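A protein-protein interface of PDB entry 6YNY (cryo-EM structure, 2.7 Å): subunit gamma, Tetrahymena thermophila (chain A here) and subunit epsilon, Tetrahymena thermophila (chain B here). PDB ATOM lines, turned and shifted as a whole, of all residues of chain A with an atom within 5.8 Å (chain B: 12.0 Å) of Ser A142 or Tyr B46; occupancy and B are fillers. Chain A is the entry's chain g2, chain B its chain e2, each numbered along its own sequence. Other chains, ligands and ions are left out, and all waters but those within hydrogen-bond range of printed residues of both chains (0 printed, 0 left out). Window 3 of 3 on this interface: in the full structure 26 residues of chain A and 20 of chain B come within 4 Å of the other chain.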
ATOM      1  N   GLY A 134       8.588   9.307  24.752  1.00  0.00           N
ATOM      2  CA  GLY A 134       8.187   9.025  23.383  1.00  0.00           C
ATOM      3  C   GLY A 134       8.540   7.602  22.986  1.00  0.00           C
ATOM      4  O   GLY A 134       9.611   7.085  23.326  1.00  0.00           O
ATOM      5  N   GLU A 135       7.625   6.960  22.255  1.00  0.00           N
ATOM      6  CA  GLU A 135       7.830   5.572  21.855  1.00  0.00           C
ATOM      7  C   GLU A 135       9.127   5.409  21.074  1.00  0.00           C
ATOM      8  O   GLU A 135       9.965   4.562  21.406  1.00  0.00           O
ATOM      9  CB  GLU A 135       6.644   5.091  21.018  1.00  0.00           C
ATOM     10  CG  GLU A 135       5.315   5.081  21.752  1.00  0.00           C
ATOM     11  CD  GLU A 135       5.230   3.982  22.793  1.00  0.00           C
ATOM     12  OE1 GLU A 135       6.235   3.270  22.994  1.00  0.00           O
ATOM     13  OE2 GLU A 135       4.152   3.828  23.404  1.00  0.00           O
ATOM     14  N   GLY A 137      11.689   7.414  20.865  1.00  0.00           N
ATOM     15  CA  GLY A 137      12.859   7.766  21.653  1.00  0.00           C
ATOM     16  C   GLY A 137      13.307   6.634  22.555  1.00  0.00           C
ATOM     17  O   GLY A 137      14.491   6.293  22.606  1.00  0.00           O
ATOM     18  N   SER A 138      12.361   6.033  23.279  1.00  0.00           N
ATOM     19  CA  SER A 138      12.706   4.951  24.194  1.00  0.00           C
ATOM     20  C   SER A 138      13.044   3.675  23.433  1.00  0.00           C
ATOM     21  O   SER A 138      14.043   3.009  23.730  1.00  0.00           O
ATOM     22  CB  SER A 138      11.550   4.706  25.162  1.00  0.00           C
ATOM     23  OG  SER A 138      10.414   4.211  24.475  1.00  0.00           O
ATOM     24  N   SER A 139      12.220   3.317  22.448  1.00  0.00           N
ATOM     25  CA  SER A 139      12.470   2.099  21.685  1.00  0.00           C
ATOM     26  C   SER A 139      13.812   2.163  20.968  1.00  0.00           C
ATOM     27  O   SER A 139      14.559   1.178  20.942  1.00  0.00           O
ATOM     28  CB  SER A 139      11.337   1.868  20.685  1.00  0.00           C
ATOM     29  OG  SER A 139      11.587   0.723  19.890  1.00  0.00           O
ATOM     30  N   GLY A 140      14.138   3.317  20.383  1.00  0.00           N
ATOM     31  CA  GLY A 140      15.402   3.447  19.680  1.00  0.00           C
ATOM     32  C   GLY A 140      16.606   3.397  20.595  1.00  0.00           C
ATOM     33  O   GLY A 140      17.686   2.966  20.182  1.00  0.00           O
ATOM     34  N   LEU A 141      16.445   3.830  21.843  1.00  0.00           N
ATOM     35  CA  LEU A 141      17.527   3.830  22.818  1.00  0.00           C
ATOM     36  C   LEU A 141      17.507   2.607  23.723  1.00  0.00           C
ATOM     37  O   LEU A 141      18.366   2.489  24.602  1.00  0.00           O
ATOM     38  CB  LEU A 141      17.463   5.104  23.667  1.00  0.00           C
ATOM     39  CG  LEU A 141      17.587   6.411  22.882  1.00  0.00           C
ATOM     40  CD1 LEU A 141      17.360   7.603  23.793  1.00  0.00           C
ATOM     41  CD2 LEU A 141      18.943   6.511  22.196  1.00  0.00           C
ATOM     42  N   SER A 142      16.553   1.695  23.528  1.00  0.00           N
ATOM     43  CA  SER A 142      16.500   0.488  24.346  1.00  0.00           C
ATOM     44  C   SER A 142      17.679  -0.432  24.050  1.00  0.00           C
ATOM     45  O   SER A 142      18.425  -0.817  24.959  1.00  0.00           O
ATOM     46  CB  SER A 142      15.179  -0.243  24.110  1.00  0.00           C
ATOM     47  OG  SER A 142      15.033  -0.607  22.749  1.00  0.00           O
ATOM     48  N   ARG A 143      17.864  -0.796  22.783  1.00  0.00           N
ATOM     49  CA  ARG A 143      18.910  -1.732  22.393  1.00  0.00           C
ATOM     50  C   ARG A 143      20.307  -1.163  22.628  1.00  0.00           C
ATOM     51  O   ARG A 143      21.182  -1.883  23.123  1.00  0.00           O
ATOM     52  CB  ARG A 143      18.746  -2.133  20.924  1.00  0.00           C
ATOM     53  CG  ARG A 143      17.463  -2.892  20.630  1.00  0.00           C
ATOM     54  CD  ARG A 143      17.020  -2.693  19.189  1.00  0.00           C
ATOM     55  NE  ARG A 143      18.055  -3.074  18.230  1.00  0.00           N
ATOM     56  CZ  ARG A 143      18.199  -4.291  17.713  1.00  0.00           C
ATOM     57  NH1 ARG A 143      17.377  -5.275  18.058  1.00  0.00           N
ATOM     58  NH2 ARG A 143      19.175  -4.528  16.847  1.00  0.00           N
ATOM     59  N   PRO A 144      20.572   0.103  22.286  1.00  0.00           N
ATOM     60  CA  PRO A 144      21.929   0.623  22.527  1.00  0.00           C
ATOM     61  C   PRO A 144      22.261   0.765  24.001  1.00  0.00           C
ATOM     62  O   PRO A 144      23.414   0.542  24.391  1.00  0.00           O
ATOM     63  CB  PRO A 144      21.921   1.982  21.811  1.00  0.00           C
ATOM     64  CG  PRO A 144      20.766   1.929  20.872  1.00  0.00           C
ATOM     65  CD  PRO A 144      19.749   1.067  21.537  1.00  0.00           C
ATOM     66  N   PHE A 145      21.287   1.130  24.838  1.00  0.00           N
ATOM     67  CA  PHE A 145      21.515   1.390  26.257  1.00  0.00           C
ATOM     68  C   PHE A 145      20.581   0.525  27.096  1.00  0.00           C
ATOM     69  O   PHE A 145      19.639   1.032  27.722  1.00  0.00           O
ATOM     70  CB  PHE A 145      21.311   2.869  26.582  1.00  0.00           C
ATOM     71  CG  PHE A 145      22.245   3.782  25.844  1.00  0.00           C
ATOM     72  CD1 PHE A 145      21.845   4.404  24.673  1.00  0.00           C
ATOM     73  CD2 PHE A 145      23.523   4.017  26.320  1.00  0.00           C
ATOM     74  CE1 PHE A 145      22.704   5.245  23.992  1.00  0.00           C
ATOM     75  CE2 PHE A 145      24.385   4.855  25.643  1.00  0.00           C
ATOM     76  CZ  PHE A 145      23.975   5.469  24.477  1.00  0.00           C
ATOM     77  N   PRO A 146      20.812  -0.783  27.134  1.00  0.00           N
ATOM     78  CA  PRO A 146      20.025  -1.643  28.020  1.00  0.00           C
ATOM     79  C   PRO A 146      20.524  -1.546  29.451  1.00  0.00           C
ATOM     80  O   PRO A 146      21.719  -1.380  29.709  1.00  0.00           O
ATOM     81  CB  PRO A 146      20.255  -3.043  27.442  1.00  0.00           C
ATOM     82  CG  PRO A 146      21.624  -2.966  26.853  1.00  0.00           C
ATOM     83  CD  PRO A 146      21.789  -1.553  26.344  1.00  0.00           C
ATOM     84  N   ASP A 147      19.589  -1.648  30.391  1.00  0.00           N
ATOM     85  CA  ASP A 147      19.835  -1.593  31.825  1.00  0.00           C
ATOM     86  C   ASP A 147      20.112  -0.160  32.276  1.00  0.00           C
ATOM     87  O   ASP A 147      20.240   0.078  33.477  1.00  0.00           O
ATOM     88  CB  ASP A 147      21.003  -2.496  32.271  1.00  0.00           C
ATOM     89  CG  ASP A 147      20.917  -2.891  33.736  1.00  0.00           C
ATOM     90  OD1 ASP A 147      20.344  -2.124  34.538  1.00  0.00           O
ATOM     91  OD2 ASP A 147      21.428  -3.975  34.086  1.00  0.00           O
ATOM     92  N   LEU A 149      18.216   2.824  30.814  1.00  0.00           N
ATOM     93  CA  LEU A 149      16.884   3.409  30.864  1.00  0.00           C
ATOM     94  C   LEU A 149      15.925   2.379  31.446  1.00  0.00           C
ATOM     95  O   LEU A 149      15.817   1.259  30.932  1.00  0.00           O
ATOM     96  CB  LEU A 149      16.432   3.856  29.473  1.00  0.00           C
ATOM     97  CG  LEU A 149      16.385   2.794  28.370  1.00  0.00           C
ATOM     98  CD1 LEU A 149      15.042   2.075  28.339  1.00  0.00           C
ATOM     99  CD2 LEU A 149      16.686   3.419  27.019  1.00  0.00           C
ATOM    100  N   LYS A 150      15.243   2.754  32.527  1.00  0.00           N
ATOM    101  CA  LYS A 150      14.360   1.851  33.250  1.00  0.00           C
ATOM    102  C   LYS A 150      12.884   2.159  33.061  1.00  0.00           C
ATOM    103  O   LYS A 150      12.066   1.239  33.121  1.00  0.00           O
ATOM    104  CB  LYS A 150      14.689   1.889  34.747  1.00  0.00           C
ATOM    105  CG  LYS A 150      16.119   1.470  35.059  1.00  0.00           C
ATOM    106  CD  LYS A 150      16.445   1.588  36.540  1.00  0.00           C
ATOM    107  CE  LYS A 150      16.537   3.040  36.982  1.00  0.00           C
ATOM    108  NZ  LYS A 150      16.945   3.164  38.406  1.00  0.00           N
ATOM    109  N   SER A 151      12.524   3.421  32.840  1.00  0.00           N
ATOM    110  CA  SER A 151      11.134   3.807  32.655  1.00  0.00           C
ATOM    111  C   SER A 151      11.056   4.936  31.638  1.00  0.00           C
ATOM    112  O   SER A 151      12.022   5.670  31.417  1.00  0.00           O
ATOM    113  CB  SER A 151      10.488   4.241  33.977  1.00  0.00           C
ATOM    114  OG  SER A 151      11.165   5.355  34.531  1.00  0.00           O
ATOM    115  N   SER A 152       9.885   5.064  31.018  1.00  0.00           N
ATOM    116  CA  SER A 152       9.652   6.097  30.020  1.00  0.00           C
ATOM    117  C   SER A 152       8.176   6.460  30.021  1.00  0.00           C
ATOM    118  O   SER A 152       7.338   5.747  30.580  1.00  0.00           O
ATOM    119  CB  SER A 152      10.090   5.639  28.627  1.00  0.00           C
ATOM    120  OG  SER A 152       9.271   4.579  28.162  1.00  0.00           O
ATOM    121  N   VAL A 154       4.999   7.562  27.417  1.00  0.00           N
ATOM    122  CA  VAL A 154       4.545   7.479  26.035  1.00  0.00           C
ATOM    123  C   VAL A 154       3.022   7.544  26.017  1.00  0.00           C
ATOM    124  O   VAL A 154       2.363   7.527  27.059  1.00  0.00           O
ATOM    125  CB  VAL A 154       5.033   6.190  25.337  1.00  0.00           C
ATOM    126  CG1 VAL A 154       6.550   6.151  25.300  1.00  0.00           C
ATOM    127  CG2 VAL A 154       4.480   4.962  26.043  1.00  0.00           C
ATOM    128  N   THR B  42       0.931   7.257  29.502  1.00  0.00           N
ATOM    129  CA  THR B  42       1.311   5.884  29.791  1.00  0.00           C
ATOM    130  C   THR B  42       2.763   5.839  30.239  1.00  0.00           C
ATOM    131  O   THR B  42       3.615   6.539  29.684  1.00  0.00           O
ATOM    132  CB  THR B  42       1.116   4.985  28.564  1.00  0.00           C
ATOM    133  OG1 THR B  42      -0.215   5.147  28.058  1.00  0.00           O
ATOM    134  CG2 THR B  42       1.337   3.522  28.925  1.00  0.00           C
ATOM    135  N   VAL B  43       3.034   5.013  31.246  1.00  0.00           N
ATOM    136  CA  VAL B  43       4.371   4.842  31.801  1.00  0.00           C
ATOM    137  C   VAL B  43       4.725   3.365  31.730  1.00  0.00           C
ATOM    138  O   VAL B  43       3.980   2.516  32.235  1.00  0.00           O
ATOM    139  CB  VAL B  43       4.460   5.352  33.250  1.00  0.00           C
ATOM    140  CG1 VAL B  43       5.881   5.209  33.771  1.00  0.00           C
ATOM    141  CG2 VAL B  43       3.995   6.797  33.333  1.00  0.00           C
ATOM    142  N   LYS B  44       5.857   3.060  31.104  1.00  0.00           N
ATOM    143  CA  LYS B  44       6.338   1.695  30.950  1.00  0.00           C
ATOM    144  C   LYS B  44       7.684   1.551  31.641  1.00  0.00           C
ATOM    145  O   LYS B  44       8.594   2.352  31.404  1.00  0.00           O
ATOM    146  CB  LYS B  44       6.478   1.321  29.472  1.00  0.00           C
ATOM    147  CG  LYS B  44       5.182   1.350  28.686  1.00  0.00           C
ATOM    148  CD  LYS B  44       5.420   0.959  27.237  1.00  0.00           C
ATOM    149  CE  LYS B  44       4.117   0.852  26.465  1.00  0.00           C
ATOM    150  NZ  LYS B  44       4.341   0.438  25.051  1.00  0.00           N
ATOM    151  N   GLN B  45       7.809   0.535  32.490  1.00  0.00           N
ATOM    152  CA  GLN B  45       9.118   0.102  32.959  1.00  0.00           C
ATOM    153  C   GLN B  45       9.774  -0.675  31.828  1.00  0.00           C
ATOM    154  O   GLN B  45       9.242  -1.697  31.381  1.00  0.00           O
ATOM    155  CB  GLN B  45       8.990  -0.751  34.217  1.00  0.00           C
ATOM    156  CG  GLN B  45       8.292  -0.037  35.360  1.00  0.00           C
ATOM    157  CD  GLN B  45       9.003   1.236  35.767  1.00  0.00           C
ATOM    158  OE1 GLN B  45      10.228   1.326  35.694  1.00  0.00           O
ATOM    159  NE2 GLN B  45       8.234   2.234  36.186  1.00  0.00           N
ATOM    160  N   TYR B  46      10.928  -0.199  31.363  1.00  0.00           N
ATOM    161  CA  TYR B  46      11.347  -0.441  29.985  1.00  0.00           C
ATOM    162  C   TYR B  46      12.265  -1.657  29.908  1.00  0.00           C
ATOM    163  O   TYR B  46      13.493  -1.563  29.934  1.00  0.00           O
ATOM    164  CB  TYR B  46      12.010   0.802  29.402  1.00  0.00           C
ATOM    165  CG  TYR B  46      11.605   1.045  27.967  1.00  0.00           C
ATOM    166  CD1 TYR B  46      12.366   0.548  26.917  1.00  0.00           C
ATOM    167  CD2 TYR B  46      10.449   1.748  27.662  1.00  0.00           C
ATOM    168  CE1 TYR B  46      11.994   0.759  25.605  1.00  0.00           C
ATOM    169  CE2 TYR B  46      10.069   1.963  26.351  1.00  0.00           C
ATOM    170  CZ  TYR B  46      10.846   1.465  25.327  1.00  0.00           C
ATOM    171  OH  TYR B  46      10.474   1.678  24.019  1.00  0.00           O
ATOM    172  N   LYS B  47      11.633  -2.820  29.818  1.00  0.00           N
ATOM    173  CA  LYS B  47      12.167  -3.969  29.108  1.00  0.00           C
ATOM    174  C   LYS B  47      11.217  -4.271  27.956  1.00  0.00           C
ATOM    175  O   LYS B  47      10.150  -3.663  27.838  1.00  0.00           O
ATOM    176  CB  LYS B  47      12.327  -5.185  30.026  1.00  0.00           C
ATOM    177  CG  LYS B  47      13.602  -5.162  30.860  1.00  0.00           C
ATOM    178  CD  LYS B  47      14.854  -5.301  30.007  1.00  0.00           C
ATOM    179  CE  LYS B  47      16.105  -5.340  30.868  1.00  0.00           C
ATOM    180  NZ  LYS B  47      17.343  -5.502  30.060  1.00  0.00           N
ATOM    181  N   GLU B  48      11.622  -5.203  27.094  1.00  0.00           N
ATOM    182  CA  GLU B  48      10.877  -5.490  25.872  1.00  0.00           C
ATOM    183  C   GLU B  48       9.368  -5.427  26.089  1.00  0.00           C
ATOM    184  O   GLU B  48       8.647  -4.846  25.270  1.00  0.00           O
ATOM    185  CB  GLU B  48      11.277  -6.862  25.323  1.00  0.00           C
ATOM    186  CG  GLU B  48      10.993  -8.028  26.258  1.00  0.00           C
ATOM    187  CD  GLU B  48      11.429  -9.359  25.676  1.00  0.00           C
ATOM    188  OE1 GLU B  48      11.990  -9.367  24.561  1.00  0.00           O
ATOM    189  OE2 GLU B  48      11.210 -10.397  26.335  1.00  0.00           O
ATOM    190  N   GLY B  49       8.875  -6.016  27.177  1.00  0.00           N
ATOM    191  CA  GLY B  49       7.461  -5.938  27.491  1.00  0.00           C
ATOM    192  C   GLY B  49       7.131  -6.077  28.964  1.00  0.00           C
ATOM    193  O   GLY B  49       6.080  -6.628  29.306  1.00  0.00           O
ATOM    194  N   LYS B  50       8.004  -5.596  29.851  1.00  0.00           N
ATOM    195  CA  LYS B  50       7.796  -5.823  31.278  1.00  0.00           C
ATOM    196  C   LYS B  50       6.481  -5.218  31.762  1.00  0.00           C
ATOM    197  O   LYS B  50       5.572  -5.939  32.189  1.00  0.00           O
ATOM    198  CB  LYS B  50       8.970  -5.263  32.083  1.00  0.00           C
ATOM    199  CG  LYS B  50       9.969  -6.321  32.517  1.00  0.00           C
ATOM    200  CD  LYS B  50      11.134  -5.720  33.283  1.00  0.00           C
ATOM    201  CE  LYS B  50      12.178  -6.777  33.605  1.00  0.00           C
ATOM    202  NZ  LYS B  50      13.407  -6.188  34.203  1.00  0.00           N
ATOM    203  N   ALA B  51       6.361  -3.893  31.701  1.00  0.00           N
ATOM    204  CA  ALA B  51       5.253  -3.205  32.348  1.00  0.00           C
ATOM    205  C   ALA B  51       4.677  -2.136  31.434  1.00  0.00           C
ATOM    206  O   ALA B  51       5.385  -1.537  30.621  1.00  0.00           O
ATOM    207  CB  ALA B  51       5.688  -2.561  33.669  1.00  0.00           C
ATOM    208  N   VAL B  52       3.374  -1.902  31.588  1.00  0.00           N
ATOM    209  CA  VAL B  52       2.672  -0.841  30.875  1.00  0.00           C
ATOM    210  C   VAL B  52       1.662  -0.235  31.838  1.00  0.00           C
ATOM    211  O   VAL B  52       0.596  -0.814  32.081  1.00  0.00           O
ATOM    212  CB  VAL B  52       1.984  -1.366  29.601  1.00  0.00           C
ATOM    213  CG1 VAL B  52       1.323  -0.223  28.847  1.00  0.00           C
ATOM    214  CG2 VAL B  52       2.984  -2.089  28.713  1.00  0.00           C
ATOM    215  N   SER B  53       1.984   0.931  32.390  1.00  0.00           N
ATOM    216  CA  SER B  53       1.114   1.610  33.342  1.00  0.00           C
ATOM    217  C   SER B  53       0.399   2.771  32.666  1.00  0.00           C
ATOM    218  O   SER B  53       1.019   3.555  31.940  1.00  0.00           O
ATOM    219  CB  SER B  53       1.918   2.119  34.538  1.00  0.00           C
ATOM    220  OG  SER B  53       1.083   2.786  35.465  1.00  0.00           O
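The side-chain carboxylate of Glu A135 is in salt-bridge range of the side-chain amino group of Lys B44.
The backbone carbonyl oxygen (O) of Val A154 sits at hydrogen-bond distance from the backbone NH (N) of Thr B42, 2.8 Å away.
The backbone carbonyl oxygen (O) of Lys A150 lies within hydrogen-bond range of the backbone NH (N) of Tyr B46.
The backbone carbonyl oxygen (O) of Lys A150 lies close to the side-chain amide oxygen (OE1) of Gln B45.
O of Lys B44 sits at hydrogen-bond distance from N of Ser A152, at 3.0 Å.
The backbone NH (N) of Ser A139 is in hydrogen-bond range of the side-chain hydroxyl (OH) of Tyr B46 (2.9 Å).
OG of Ser A138 sits at hydrogen-bond distance from OH of Tyr B46 (2.6 Å).
The side-chain hydroxyl (OG) of Ser A138 lies within hydrogen-bond range of the backbone carbonyl oxygen (O) of Glu A135 (3.1 Å).
The side-chain hydroxyl (OG) of Ser A138 lies within hydrogen-bond range of the backbone carbonyl oxygen (O) of Gly A134.
The backbone NH of Ser B53 sits at hydrogen-bond distance from the backbone carbonyl oxygen of Val B43 (2.6 Å).
The backbone carbonyl oxygen of Ser A139 is in hydrogen-bond range of the side-chain hydroxyl of Ser A142 (2.6 Å).
Among the printed residues, pairs that only touch across the chains: Glu A135 with Tyr B46, Ser A142 with Tyr B46, Leu A149 with Tyr B46, Ser A151 with Lys B44, Ser A151 with Gln B45, Ser A152 with Thr B42, Ser A152 with Val B43 and Ser A152 with Tyr B46.
Of chain B, only Tyr B46 comes within 4 Å of Ser A142.
Of chain A, only Glu A135, Ser A138, Ser A139, Ser A142, Leu A149, Lys A150 and Ser A152 come within 4 Å of Tyr B46.
Gly A134 touches none of the printed residues of chain B.
Glu A135 touches just these residues of chain B: Lys B44 (3.8 Å) and Tyr B46 (3.9 Å).
Gly A137 touches none of the printed residues of chain B.
No residue of chain B comes within 4 Å of Gly A140.
No residue of chain B comes within 4 Å of Leu A141.
No residue of chain B comes within 4 Å of Pro A144.
No residue of chain B comes within 4 Å of Pro A146.
Leu A149 touches just one residue of chain B: Tyr B46 (3.4 Å).
Of chain B, only Lys B44 and Gln B45 come within 4 Å of Ser A151.
Printed residues of chain A within 4 Å of Thr B42: Ser A152 and Val A154.
Printed residues of chain B within 4 Å of Lys A150: Gln B45 (3.2 Å) and Tyr B46 (2.5 Å).
Of the 18 printed residues of chain A, 9 touch a printed residue of chain B.
Hydrophobic or aromatic side chains of chain A that line the printed part of chain B: Leu A149.
Of the 12 printed residues of chain B, 5 touch a printed residue of chain A.
Printed residues of chain B that touch a printed residue of chain A: Thr B42, Val B43, Lys B44, Gln B45 and Tyr B46.
Hydrophobic or aromatic side chains of chain B within 4 Å of the printed part of chain A: Val B43 and Tyr B46.
Among the printed residues, Asp or Glu carboxylates within 4 Å of a Lys or Arg side-chain nitrogen of the other chain: Glu A135 with Lys B44.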
